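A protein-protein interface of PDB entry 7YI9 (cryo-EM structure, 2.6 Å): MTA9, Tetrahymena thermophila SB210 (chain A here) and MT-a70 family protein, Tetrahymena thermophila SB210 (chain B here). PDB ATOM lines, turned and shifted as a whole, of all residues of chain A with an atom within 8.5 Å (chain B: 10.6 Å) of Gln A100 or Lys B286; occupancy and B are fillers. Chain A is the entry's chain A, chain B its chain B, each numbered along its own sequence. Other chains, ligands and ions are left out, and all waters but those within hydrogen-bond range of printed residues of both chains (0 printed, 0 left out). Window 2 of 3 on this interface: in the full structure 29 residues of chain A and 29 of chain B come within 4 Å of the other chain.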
ATOM      1  N   ASP A  98      -4.134   9.436 -21.746  1.00  0.00           N
ATOM      2  CA  ASP A  98      -5.280   8.577 -21.477  1.00  0.00           C
ATOM      3  C   ASP A  98      -4.838   7.142 -21.221  1.00  0.00           C
ATOM      4  O   ASP A  98      -3.894   6.906 -20.469  1.00  0.00           O
ATOM      5  CB  ASP A  98      -6.269   8.628 -22.641  1.00  0.00           C
ATOM      6  CG  ASP A  98      -7.220   9.805 -22.544  1.00  0.00           C
ATOM      7  OD1 ASP A  98      -8.101   9.789 -21.659  1.00  0.00           O
ATOM      8  OD2 ASP A  98      -7.085  10.749 -23.351  1.00  0.00           O
ATOM      9  N   ASN A  99      -5.531   6.187 -21.845  1.00  0.00           N
ATOM     10  CA  ASN A  99      -5.142   4.787 -21.712  1.00  0.00           C
ATOM     11  C   ASN A  99      -3.746   4.545 -22.263  1.00  0.00           C
ATOM     12  O   ASN A  99      -2.960   3.796 -21.672  1.00  0.00           O
ATOM     13  CB  ASN A  99      -6.140   3.888 -22.435  1.00  0.00           C
ATOM     14  CG  ASN A  99      -7.468   3.824 -21.746  1.00  0.00           C
ATOM     15  OD1 ASN A  99      -8.484   4.219 -22.305  1.00  0.00           O
ATOM     16  ND2 ASN A  99      -7.475   3.324 -20.522  1.00  0.00           N
ATOM     17  N   GLN A 100      -3.431   5.160 -23.405  1.00  0.00           N
ATOM     18  CA  GLN A 100      -2.195   4.902 -24.141  1.00  0.00           C
ATOM     19  C   GLN A 100      -2.125   3.448 -24.604  1.00  0.00           C
ATOM     20  O   GLN A 100      -1.043   2.891 -24.796  1.00  0.00           O
ATOM     21  CB  GLN A 100      -0.958   5.275 -23.320  1.00  0.00           C
ATOM     22  CG  GLN A 100      -0.987   6.681 -22.761  1.00  0.00           C
ATOM     23  CD  GLN A 100      -0.584   7.721 -23.785  1.00  0.00           C
ATOM     24  OE1 GLN A 100      -0.164   7.387 -24.892  1.00  0.00           O
ATOM     25  NE2 GLN A 100      -0.712   8.990 -23.422  1.00  0.00           N
ATOM     26  N   LEU A 101      -3.289   2.830 -24.798  1.00  0.00           N
ATOM     27  CA  LEU A 101      -3.355   1.459 -25.287  1.00  0.00           C
ATOM     28  C   LEU A 101      -2.853   1.314 -26.716  1.00  0.00           C
ATOM     29  O   LEU A 101      -2.570   0.191 -27.142  1.00  0.00           O
ATOM     30  CB  LEU A 101      -4.787   0.928 -25.193  1.00  0.00           C
ATOM     31  CG  LEU A 101      -5.306   0.624 -23.791  1.00  0.00           C
ATOM     32  CD1 LEU A 101      -6.712   0.067 -23.861  1.00  0.00           C
ATOM     33  CD2 LEU A 101      -4.383  -0.339 -23.075  1.00  0.00           C
ATOM     34  N   SER A 102      -2.743   2.410 -27.466  1.00  0.00           N
ATOM     35  CA  SER A 102      -2.096   2.363 -28.768  1.00  0.00           C
ATOM     36  C   SER A 102      -0.620   2.008 -28.662  1.00  0.00           C
ATOM     37  O   SER A 102      -0.044   1.509 -29.634  1.00  0.00           O
ATOM     38  CB  SER A 102      -2.253   3.706 -29.484  1.00  0.00           C
ATOM     39  OG  SER A 102      -1.581   3.703 -30.731  1.00  0.00           O
ATOM     40  N   LEU A 103      -0.005   2.252 -27.507  1.00  0.00           N
ATOM     41  CA  LEU A 103       1.389   1.912 -27.268  1.00  0.00           C
ATOM     42  C   LEU A 103       1.559   0.670 -26.405  1.00  0.00           C
ATOM     43  O   LEU A 103       2.558  -0.039 -26.552  1.00  0.00           O
ATOM     44  CB  LEU A 103       2.111   3.089 -26.605  1.00  0.00           C
ATOM     45  CG  LEU A 103       3.640   3.079 -26.665  1.00  0.00           C
ATOM     46  CD1 LEU A 103       4.123   3.301 -28.088  1.00  0.00           C
ATOM     47  CD2 LEU A 103       4.226   4.122 -25.729  1.00  0.00           C
ATOM     48  N   LEU A 104       0.608   0.387 -25.516  1.00  0.00           N
ATOM     49  CA  LEU A 104       0.685  -0.790 -24.662  1.00  0.00           C
ATOM     50  C   LEU A 104       0.258  -2.067 -25.372  1.00  0.00           C
ATOM     51  O   LEU A 104       0.506  -3.159 -24.848  1.00  0.00           O
ATOM     52  CB  LEU A 104      -0.176  -0.593 -23.414  1.00  0.00           C
ATOM     53  CG  LEU A 104       0.154   0.601 -22.519  1.00  0.00           C
ATOM     54  CD1 LEU A 104      -0.822   0.672 -21.365  1.00  0.00           C
ATOM     55  CD2 LEU A 104       1.576   0.515 -22.009  1.00  0.00           C
ATOM     56  N   LEU A 105      -0.379  -1.962 -26.538  1.00  0.00           N
ATOM     57  CA  LEU A 105      -0.788  -3.125 -27.314  1.00  0.00           C
ATOM     58  C   LEU A 105      -0.231  -3.069 -28.731  1.00  0.00           C
ATOM     59  O   LEU A 105      -0.760  -3.732 -29.624  1.00  0.00           O
ATOM     60  CB  LEU A 105      -2.314  -3.241 -27.346  1.00  0.00           C
ATOM     61  CG  LEU A 105      -3.014  -3.618 -26.039  1.00  0.00           C
ATOM     62  CD1 LEU A 105      -4.499  -3.312 -26.120  1.00  0.00           C
ATOM     63  CD2 LEU A 105      -2.792  -5.080 -25.700  1.00  0.00           C
ATOM     64  N   LYS A 106       0.834  -2.294 -28.947  1.00  0.00           N
ATOM     65  CA  LYS A 106       1.366  -2.075 -30.288  1.00  0.00           C
ATOM     66  C   LYS A 106       2.014  -3.318 -30.878  1.00  0.00           C
ATOM     67  O   LYS A 106       1.992  -3.490 -32.100  1.00  0.00           O
ATOM     68  CB  LYS A 106       2.379  -0.933 -30.265  1.00  0.00           C
ATOM     69  CG  LYS A 106       2.651  -0.323 -31.625  1.00  0.00           C
ATOM     70  CD  LYS A 106       3.546   0.896 -31.510  1.00  0.00           C
ATOM     71  CE  LYS A 106       2.724   2.163 -31.344  1.00  0.00           C
ATOM     72  NZ  LYS A 106       1.914   2.469 -32.555  1.00  0.00           N
ATOM     73  N   LEU A 216      -5.500  -7.636 -19.794  1.00  0.00           N
ATOM     74  CA  LEU A 216      -6.689  -6.815 -19.955  1.00  0.00           C
ATOM     75  C   LEU A 216      -7.814  -7.683 -20.497  1.00  0.00           C
ATOM     76  O   LEU A 216      -7.608  -8.465 -21.427  1.00  0.00           O
ATOM     77  CB  LEU A 216      -6.433  -5.646 -20.909  1.00  0.00           C
ATOM     78  CG  LEU A 216      -5.280  -4.690 -20.604  1.00  0.00           C
ATOM     79  CD1 LEU A 216      -4.983  -3.836 -21.815  1.00  0.00           C
ATOM     80  CD2 LEU A 216      -5.600  -3.815 -19.408  1.00  0.00           C
ATOM     81  N   LEU A 335      -9.639   1.031 -31.584  1.00  0.00           N
ATOM     82  CA  LEU A 335      -8.748   1.284 -30.459  1.00  0.00           C
ATOM     83  C   LEU A 335      -8.725   2.767 -30.099  1.00  0.00           C
ATOM     84  O   LEU A 335      -7.885   3.211 -29.309  1.00  0.00           O
ATOM     85  CB  LEU A 335      -7.347   0.758 -30.786  1.00  0.00           C
ATOM     86  CG  LEU A 335      -6.206   0.810 -29.767  1.00  0.00           C
ATOM     87  CD1 LEU A 335      -6.570  -0.050 -28.565  1.00  0.00           C
ATOM     88  CD2 LEU A 335      -4.886   0.366 -30.378  1.00  0.00           C
ATOM     89  N   LEU A 338     -12.443   3.495 -26.944  1.00  0.00           N
ATOM     90  CA  LEU A 338     -12.244   3.225 -25.528  1.00  0.00           C
ATOM     91  C   LEU A 338     -11.032   3.956 -24.970  1.00  0.00           C
ATOM     92  O   LEU A 338     -10.611   3.671 -23.847  1.00  0.00           O
ATOM     93  CB  LEU A 338     -12.106   1.719 -25.284  1.00  0.00           C
ATOM     94  CG  LEU A 338     -10.793   1.027 -25.658  1.00  0.00           C
ATOM     95  CD1 LEU A 338     -10.718  -0.322 -24.980  1.00  0.00           C
ATOM     96  CD2 LEU A 338     -10.650   0.867 -27.159  1.00  0.00           C
ATOM     97  N   LYS A 339     -10.465   4.892 -25.733  1.00  0.00           N
ATOM     98  CA  LYS A 339      -9.316   5.660 -25.271  1.00  0.00           C
ATOM     99  C   LYS A 339      -9.645   6.532 -24.066  1.00  0.00           C
ATOM    100  O   LYS A 339      -8.749   6.834 -23.273  1.00  0.00           O
ATOM    101  CB  LYS A 339      -8.780   6.521 -26.415  1.00  0.00           C
ATOM    102  CG  LYS A 339      -7.512   7.284 -26.092  1.00  0.00           C
ATOM    103  CD  LYS A 339      -6.382   6.324 -25.769  1.00  0.00           C
ATOM    104  CE  LYS A 339      -5.969   5.531 -26.996  1.00  0.00           C
ATOM    105  NZ  LYS A 339      -4.833   4.621 -26.708  1.00  0.00           N
ATOM    106  N   SER A 340     -10.903   6.941 -23.908  1.00  0.00           N
ATOM    107  CA  SER A 340     -11.285   7.778 -22.779  1.00  0.00           C
ATOM    108  C   SER A 340     -11.472   6.985 -21.491  1.00  0.00           C
ATOM    109  O   SER A 340     -11.504   7.586 -20.412  1.00  0.00           O
ATOM    110  CB  SER A 340     -12.571   8.540 -23.105  1.00  0.00           C
ATOM    111  OG  SER A 340     -13.626   7.647 -23.415  1.00  0.00           O
ATOM    112  N   THR A 341     -11.591   5.664 -21.579  1.00  0.00           N
ATOM    113  CA  THR A 341     -11.817   4.834 -20.406  1.00  0.00           C
ATOM    114  C   THR A 341     -10.591   4.845 -19.495  1.00  0.00           C
ATOM    115  O   THR A 341      -9.467   5.121 -19.918  1.00  0.00           O
ATOM    116  CB  THR A 341     -12.157   3.402 -20.831  1.00  0.00           C
ATOM    117  OG1 THR A 341     -13.117   3.437 -21.891  1.00  0.00           O
ATOM    118  CG2 THR A 341     -12.748   2.608 -19.676  1.00  0.00           C
ATOM    119  N   ILE A 343      -7.824   2.959 -17.433  1.00  0.00           N
ATOM    120  CA  ILE A 343      -7.173   1.677 -17.685  1.00  0.00           C
ATOM    121  C   ILE A 343      -7.363   0.717 -16.518  1.00  0.00           C
ATOM    122  O   ILE A 343      -7.463  -0.499 -16.718  1.00  0.00           O
ATOM    123  CB  ILE A 343      -5.682   1.884 -18.017  1.00  0.00           C
ATOM    124  CG1 ILE A 343      -5.061   0.576 -18.510  1.00  0.00           C
ATOM    125  CG2 ILE A 343      -4.922   2.430 -16.819  1.00  0.00           C
ATOM    126  CD1 ILE A 343      -3.765   0.764 -19.244  1.00  0.00           C
ATOM    127  N   LEU A 346     -10.234  -1.571 -17.024  1.00  0.00           N
ATOM    128  CA  LEU A 346     -10.152  -2.605 -18.047  1.00  0.00           C
ATOM    129  C   LEU A 346      -9.328  -3.811 -17.617  1.00  0.00           C
ATOM    130  O   LEU A 346      -9.369  -4.839 -18.301  1.00  0.00           O
ATOM    131  CB  LEU A 346      -9.561  -2.027 -19.338  1.00  0.00           C
ATOM    132  CG  LEU A 346     -10.365  -0.915 -20.005  1.00  0.00           C
ATOM    133  CD1 LEU A 346      -9.526  -0.199 -21.052  1.00  0.00           C
ATOM    134  CD2 LEU A 346     -11.635  -1.477 -20.615  1.00  0.00           C
ATOM    135  N   PHE A 387       1.634  -6.275 -22.015  1.00  0.00           N
ATOM    136  CA  PHE A 387       0.190  -6.143 -21.882  1.00  0.00           C
ATOM    137  C   PHE A 387      -0.496  -6.973 -22.955  1.00  0.00           C
ATOM    138  O   PHE A 387      -0.115  -6.916 -24.127  1.00  0.00           O
ATOM    139  CB  PHE A 387      -0.236  -4.679 -21.995  1.00  0.00           C
ATOM    140  CG  PHE A 387      -0.085  -3.905 -20.720  1.00  0.00           C
ATOM    141  CD1 PHE A 387       1.110  -3.288 -20.409  1.00  0.00           C
ATOM    142  CD2 PHE A 387      -1.138  -3.803 -19.830  1.00  0.00           C
ATOM    143  CE1 PHE A 387       1.252  -2.579 -19.240  1.00  0.00           C
ATOM    144  CE2 PHE A 387      -0.999  -3.092 -18.658  1.00  0.00           C
ATOM    145  CZ  PHE A 387       0.199  -2.479 -18.363  1.00  0.00           C
ATOM    146  N   TRP B 278       4.089  -4.052  -8.511  1.00  0.00           N
ATOM    147  CA  TRP B 278       3.827  -2.637  -8.731  1.00  0.00           C
ATOM    148  C   TRP B 278       4.486  -2.249 -10.050  1.00  0.00           C
ATOM    149  O   TRP B 278       5.716  -2.195 -10.144  1.00  0.00           O
ATOM    150  CB  TRP B 278       4.344  -1.793  -7.567  1.00  0.00           C
ATOM    151  CG  TRP B 278       4.396  -0.320  -7.850  1.00  0.00           C
ATOM    152  CD1 TRP B 278       3.502   0.408  -8.577  1.00  0.00           C
ATOM    153  CD2 TRP B 278       5.395   0.601  -7.406  1.00  0.00           C
ATOM    154  NE1 TRP B 278       3.885   1.722  -8.619  1.00  0.00           N
ATOM    155  CE2 TRP B 278       5.044   1.868  -7.906  1.00  0.00           C
ATOM    156  CE3 TRP B 278       6.551   0.477  -6.632  1.00  0.00           C
ATOM    157  CZ2 TRP B 278       5.808   3.004  -7.658  1.00  0.00           C
ATOM    158  CZ3 TRP B 278       7.307   1.604  -6.388  1.00  0.00           C
ATOM    159  CH2 TRP B 278       6.933   2.851  -6.899  1.00  0.00           C
ATOM    160  N   VAL B 279       3.667  -1.986 -11.062  1.00  0.00           N
ATOM    161  CA  VAL B 279       4.151  -1.551 -12.366  1.00  0.00           C
ATOM    162  C   VAL B 279       4.169  -0.031 -12.385  1.00  0.00           C
ATOM    163  O   VAL B 279       3.150   0.615 -12.118  1.00  0.00           O
ATOM    164  CB  VAL B 279       3.271  -2.111 -13.495  1.00  0.00           C
ATOM    165  CG1 VAL B 279       3.907  -1.849 -14.845  1.00  0.00           C
ATOM    166  CG2 VAL B 279       3.033  -3.596 -13.295  1.00  0.00           C
ATOM    167  N   LYS B 280       5.324   0.543 -12.698  1.00  0.00           N
ATOM    168  CA  LYS B 280       5.506   1.983 -12.594  1.00  0.00           C
ATOM    169  C   LYS B 280       4.942   2.691 -13.817  1.00  0.00           C
ATOM    170  O   LYS B 280       5.190   2.285 -14.956  1.00  0.00           O
ATOM    171  CB  LYS B 280       6.985   2.317 -12.428  1.00  0.00           C
ATOM    172  CG  LYS B 280       7.564   1.792 -11.142  1.00  0.00           C
ATOM    173  CD  LYS B 280       9.064   1.942 -11.103  1.00  0.00           C
ATOM    174  CE  LYS B 280       9.582   1.435  -9.783  1.00  0.00           C
ATOM    175  NZ  LYS B 280       8.996   0.100  -9.530  1.00  0.00           N
ATOM    176  N   LYS B 281       4.190   3.756 -13.573  1.00  0.00           N
ATOM    177  CA  LYS B 281       3.600   4.576 -14.617  1.00  0.00           C
ATOM    178  C   LYS B 281       4.319   5.919 -14.690  1.00  0.00           C
ATOM    179  O   LYS B 281       4.991   6.342 -13.749  1.00  0.00           O
ATOM    180  CB  LYS B 281       2.110   4.786 -14.344  1.00  0.00           C
ATOM    181  CG  LYS B 281       1.292   5.157 -15.554  1.00  0.00           C
ATOM    182  CD  LYS B 281      -0.038   5.751 -15.143  1.00  0.00           C
ATOM    183  CE  LYS B 281      -0.943   4.708 -14.533  1.00  0.00           C
ATOM    184  NZ  LYS B 281      -2.319   5.229 -14.337  1.00  0.00           N
ATOM    185  N   THR B 282       4.179   6.582 -15.832  1.00  0.00           N
ATOM    186  CA  THR B 282       4.691   7.930 -16.006  1.00  0.00           C
ATOM    187  C   THR B 282       3.548   8.933 -15.870  1.00  0.00           C
ATOM    188  O   THR B 282       2.383   8.572 -15.691  1.00  0.00           O
ATOM    189  CB  THR B 282       5.393   8.075 -17.357  1.00  0.00           C
ATOM    190  OG1 THR B 282       4.421   8.063 -18.409  1.00  0.00           O
ATOM    191  CG2 THR B 282       6.378   6.939 -17.572  1.00  0.00           C
ATOM    192  N   VAL B 283       3.893  10.220 -15.953  1.00  0.00           N
ATOM    193  CA  VAL B 283       2.868  11.257 -15.931  1.00  0.00           C
ATOM    194  C   VAL B 283       1.986  11.160 -17.170  1.00  0.00           C
ATOM    195  O   VAL B 283       0.775  11.408 -17.110  1.00  0.00           O
ATOM    196  CB  VAL B 283       3.514  12.647 -15.797  1.00  0.00           C
ATOM    197  CG1 VAL B 283       4.018  12.856 -14.380  1.00  0.00           C
ATOM    198  CG2 VAL B 283       4.645  12.807 -16.799  1.00  0.00           C
ATOM    199  N   ASN B 284       2.575  10.794 -18.311  1.00  0.00           N
ATOM    200  CA  ASN B 284       1.804  10.613 -19.534  1.00  0.00           C
ATOM    201  C   ASN B 284       0.898   9.389 -19.477  1.00  0.00           C
ATOM    202  O   ASN B 284      -0.048   9.301 -20.266  1.00  0.00           O
ATOM    203  CB  ASN B 284       2.744  10.499 -20.733  1.00  0.00           C
ATOM    204  CG  ASN B 284       3.545  11.761 -20.966  1.00  0.00           C
ATOM    205  OD1 ASN B 284       4.768  11.765 -20.834  1.00  0.00           O
ATOM    206  ND2 ASN B 284       2.857  12.844 -21.312  1.00  0.00           N
ATOM    207  N   GLY B 285       1.161   8.452 -18.573  1.00  0.00           N
ATOM    208  CA  GLY B 285       0.406   7.220 -18.500  1.00  0.00           C
ATOM    209  C   GLY B 285       1.069   6.013 -19.124  1.00  0.00           C
ATOM    210  O   GLY B 285       0.401   4.987 -19.297  1.00  0.00           O
ATOM    211  N   LYS B 286       2.352   6.102 -19.470  1.00  0.00           N
ATOM    212  CA  LYS B 286       3.083   5.019 -20.106  1.00  0.00           C
ATOM    213  C   LYS B 286       3.905   4.249 -19.074  1.00  0.00           C
ATOM    214  O   LYS B 286       4.018   4.637 -17.909  1.00  0.00           O
ATOM    215  CB  LYS B 286       3.978   5.565 -21.219  1.00  0.00           C
ATOM    216  CG  LYS B 286       3.221   6.075 -22.430  1.00  0.00           C
ATOM    217  CD  LYS B 286       4.079   6.995 -23.274  1.00  0.00           C
ATOM    218  CE  LYS B 286       3.233   8.053 -23.956  1.00  0.00           C
ATOM    219  NZ  LYS B 286       3.870   8.562 -25.203  1.00  0.00           N
ATOM    220  N   ILE B 287       4.489   3.135 -19.518  1.00  0.00           N
ATOM    221  CA  ILE B 287       5.326   2.316 -18.649  1.00  0.00           C
ATOM    222  C   ILE B 287       6.672   2.996 -18.446  1.00  0.00           C
ATOM    223  O   ILE B 287       7.310   3.448 -19.405  1.00  0.00           O
ATOM    224  CB  ILE B 287       5.506   0.912 -19.242  1.00  0.00           C
ATOM    225  CG1 ILE B 287       4.158   0.224 -19.417  1.00  0.00           C
ATOM    226  CG2 ILE B 287       6.407   0.071 -18.356  1.00  0.00           C
ATOM    227  CD1 ILE B 287       3.592  -0.289 -18.136  1.00  0.00           C
ATOM    228  N   ALA B 288       7.114   3.066 -17.194  1.00  0.00           N
ATOM    229  CA  ALA B 288       8.438   3.578 -16.869  1.00  0.00           C
ATOM    230  C   ALA B 288       9.465   2.468 -17.051  1.00  0.00           C
ATOM    231  O   ALA B 288       9.269   1.349 -16.566  1.00  0.00           O
ATOM    232  CB  ALA B 288       8.477   4.114 -15.438  1.00  0.00           C
ATOM    233  N   LYS B 289      10.555   2.781 -17.743  1.00  0.00           N
ATOM    234  CA  LYS B 289      11.569   1.787 -18.069  1.00  0.00           C
ATOM    235  C   LYS B 289      12.459   1.548 -16.851  1.00  0.00           C
ATOM    236  O   LYS B 289      12.176   2.004 -15.740  1.00  0.00           O
ATOM    237  CB  LYS B 289      12.381   2.228 -19.284  1.00  0.00           C
ATOM    238  CG  LYS B 289      11.743   1.929 -20.635  1.00  0.00           C
ATOM    239  CD  LYS B 289      10.578   2.858 -20.925  1.00  0.00           C
ATOM    240  CE  LYS B 289      11.061   4.280 -21.169  1.00  0.00           C
ATOM    241  NZ  LYS B 289       9.941   5.199 -21.518  1.00  0.00           N
ATOM    242  N   GLY B 290      13.547   0.822 -17.048  1.00  0.00           N
ATOM    243  CA  GLY B 290      14.467   0.567 -15.964  1.00  0.00           C
ATOM    244  C   GLY B 290      15.719  -0.110 -16.460  1.00  0.00           C
ATOM    245  O   GLY B 290      15.994  -0.141 -17.660  1.00  0.00           O
ATOM    246  N   ALA B 298      10.765  -3.176 -15.004  1.00  0.00           N
ATOM    247  CA  ALA B 298       9.690  -2.192 -14.992  1.00  0.00           C
ATOM    248  C   ALA B 298       8.696  -2.452 -13.866  1.00  0.00           C
ATOM    249  O   ALA B 298       7.570  -1.949 -13.921  1.00  0.00           O
ATOM    250  CB  ALA B 298       8.957  -2.169 -16.334  1.00  0.00           C
ATOM    251  N   ILE B 324      -0.318  -3.112  -9.252  1.00  0.00           N
ATOM    252  CA  ILE B 324      -0.517  -1.692  -8.996  1.00  0.00           C
ATOM    253  C   ILE B 324       0.123  -0.942 -10.151  1.00  0.00           C
ATOM    254  O   ILE B 324       1.339  -1.026 -10.359  1.00  0.00           O
ATOM    255  CB  ILE B 324       0.084  -1.255  -7.654  1.00  0.00           C
ATOM    256  CG1 ILE B 324      -0.654  -1.920  -6.494  1.00  0.00           C
ATOM    257  CG2 ILE B 324       0.034   0.257  -7.517  1.00  0.00           C
ATOM    258  CD1 ILE B 324      -0.047  -1.635  -5.145  1.00  0.00           C
ATOM    259  N   PHE B 325      -0.685  -0.209 -10.905  1.00  0.00           N
ATOM    260  CA  PHE B 325      -0.211   0.572 -12.043  1.00  0.00           C
ATOM    261  C   PHE B 325      -0.341   2.043 -11.649  1.00  0.00           C
ATOM    262  O   PHE B 325      -1.363   2.681 -11.896  1.00  0.00           O
ATOM    263  CB  PHE B 325      -1.004   0.217 -13.305  1.00  0.00           C
ATOM    264  CG  PHE B 325      -0.429   0.783 -14.571  1.00  0.00           C
ATOM    265  CD1 PHE B 325       0.932   0.772 -14.794  1.00  0.00           C
ATOM    266  CD2 PHE B 325      -1.257   1.285 -15.557  1.00  0.00           C
ATOM    267  CE1 PHE B 325       1.460   1.284 -15.959  1.00  0.00           C
ATOM    268  CE2 PHE B 325      -0.735   1.791 -16.728  1.00  0.00           C
ATOM    269  CZ  PHE B 325       0.626   1.788 -16.929  1.00  0.00           C
ATOM    270  N   SER B 326       0.708   2.573 -11.023  1.00  0.00           N
ATOM    271  CA  SER B 326       0.675   3.904 -10.436  1.00  0.00           C
ATOM    272  C   SER B 326       1.961   4.645 -10.763  1.00  0.00           C
ATOM    273  O   SER B 326       2.993   4.044 -11.070  1.00  0.00           O
ATOM    274  CB  SER B 326       0.478   3.848  -8.919  1.00  0.00           C
ATOM    275  OG  SER B 326      -0.814   3.379  -8.590  1.00  0.00           O
ATOM    276  N   GLU B 327       1.885   5.970 -10.686  1.00  0.00           N
ATOM    277  CA  GLU B 327       3.014   6.817 -11.038  1.00  0.00           C
ATOM    278  C   GLU B 327       4.127   6.709 -10.004  1.00  0.00           C
ATOM    279  O   GLU B 327       3.893   6.425  -8.827  1.00  0.00           O
ATOM    280  CB  GLU B 327       2.571   8.274 -11.170  1.00  0.00           C
ATOM    281  CG  GLU B 327       1.436   8.504 -12.159  1.00  0.00           C
ATOM    282  CD  GLU B 327       0.062   8.302 -11.546  1.00  0.00           C
ATOM    283  OE1 GLU B 327      -0.059   7.508 -10.591  1.00  0.00           O
ATOM    284  OE2 GLU B 327      -0.900   8.941 -12.024  1.00  0.00           O
ATOM    285  N   ARG B 328       5.351   6.951 -10.460  1.00  0.00           N
ATOM    286  CA  ARG B 328       6.521   6.904  -9.595  1.00  0.00           C
ATOM    287  C   ARG B 328       6.623   8.202  -8.801  1.00  0.00           C
ATOM    288  O   ARG B 328       6.791   9.281  -9.380  1.00  0.00           O
ATOM    289  CB  ARG B 328       7.779   6.676 -10.429  1.00  0.00           C
ATOM    290  CG  ARG B 328       8.942   6.085  -9.660  1.00  0.00           C
ATOM    291  CD  ARG B 328      10.049   5.645 -10.598  1.00  0.00           C
ATOM    292  NE  ARG B 328      10.077   6.453 -11.812  1.00  0.00           N
ATOM    293  CZ  ARG B 328      10.731   6.123 -12.917  1.00  0.00           C
ATOM    294  NH1 ARG B 328      11.435   5.006 -12.997  1.00  0.00           N
ATOM    295  NH2 ARG B 328      10.676   6.935 -13.968  1.00  0.00           N
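The side-chain hydroxyl (OG1) of Thr B282 lies within hydrogen-bond range of the backbone NH (N) of Lys B286, 3.0 Å away.
The side-chain hydroxyl of Thr B282 sits close to the backbone NH of Asn B284, 3.3 Å away.
The side-chain amide nitrogen (NE2) of Gln A100 is in hydrogen-bond range of the backbone carbonyl oxygen (O) of Asn B284 (3.2 Å).
Among the printed residues, pairs that only touch across the chains: Gln A100 with Lys B286, Leu A103 with Lys B286, Leu A104 with Ile B287 and Phe A387 with Ile B287.
No residue of chain B comes within 4 Å of Asn A99.
No residue of chain B comes within 4 Å of Leu A101.
No residue of chain B comes within 4 Å of Ser A102.
Of chain B, only Lys B286 comes within 4 Å of Leu A103.
Leu A104 touches just one residue of chain B: Ile B287.
Printed residues of chain B within 4 Å of Phe A387: Ile B287 (3.5 Å).
Of the printed residues of chain A, Asn B284 touches Gln A100 (3.2 Å).
Of chain A, only Gln A100 and Leu A103 come within 4 Å of Lys B286.
Of the printed residues of chain A, Ile B287 touches Leu A104 and Phe A387.
The nearest residue of chain A that does not touch Lys B286 is Leu A104 (5.1 Å).
Printed residues of chain A that touch a printed residue of chain B: Gln A100, Leu A103, Leu A104 and Phe A387.
Hydrophobic or aromatic side chains of chain A that line the printed part of chain B: Leu A103, Leu A104 and Phe A387.
Hydrophobic or aromatic side chains of chain B that line the printed part of chain A: Ile B287.
Along chain B the printed residues that touch a printed residue of chain A span positions 284 to 287.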
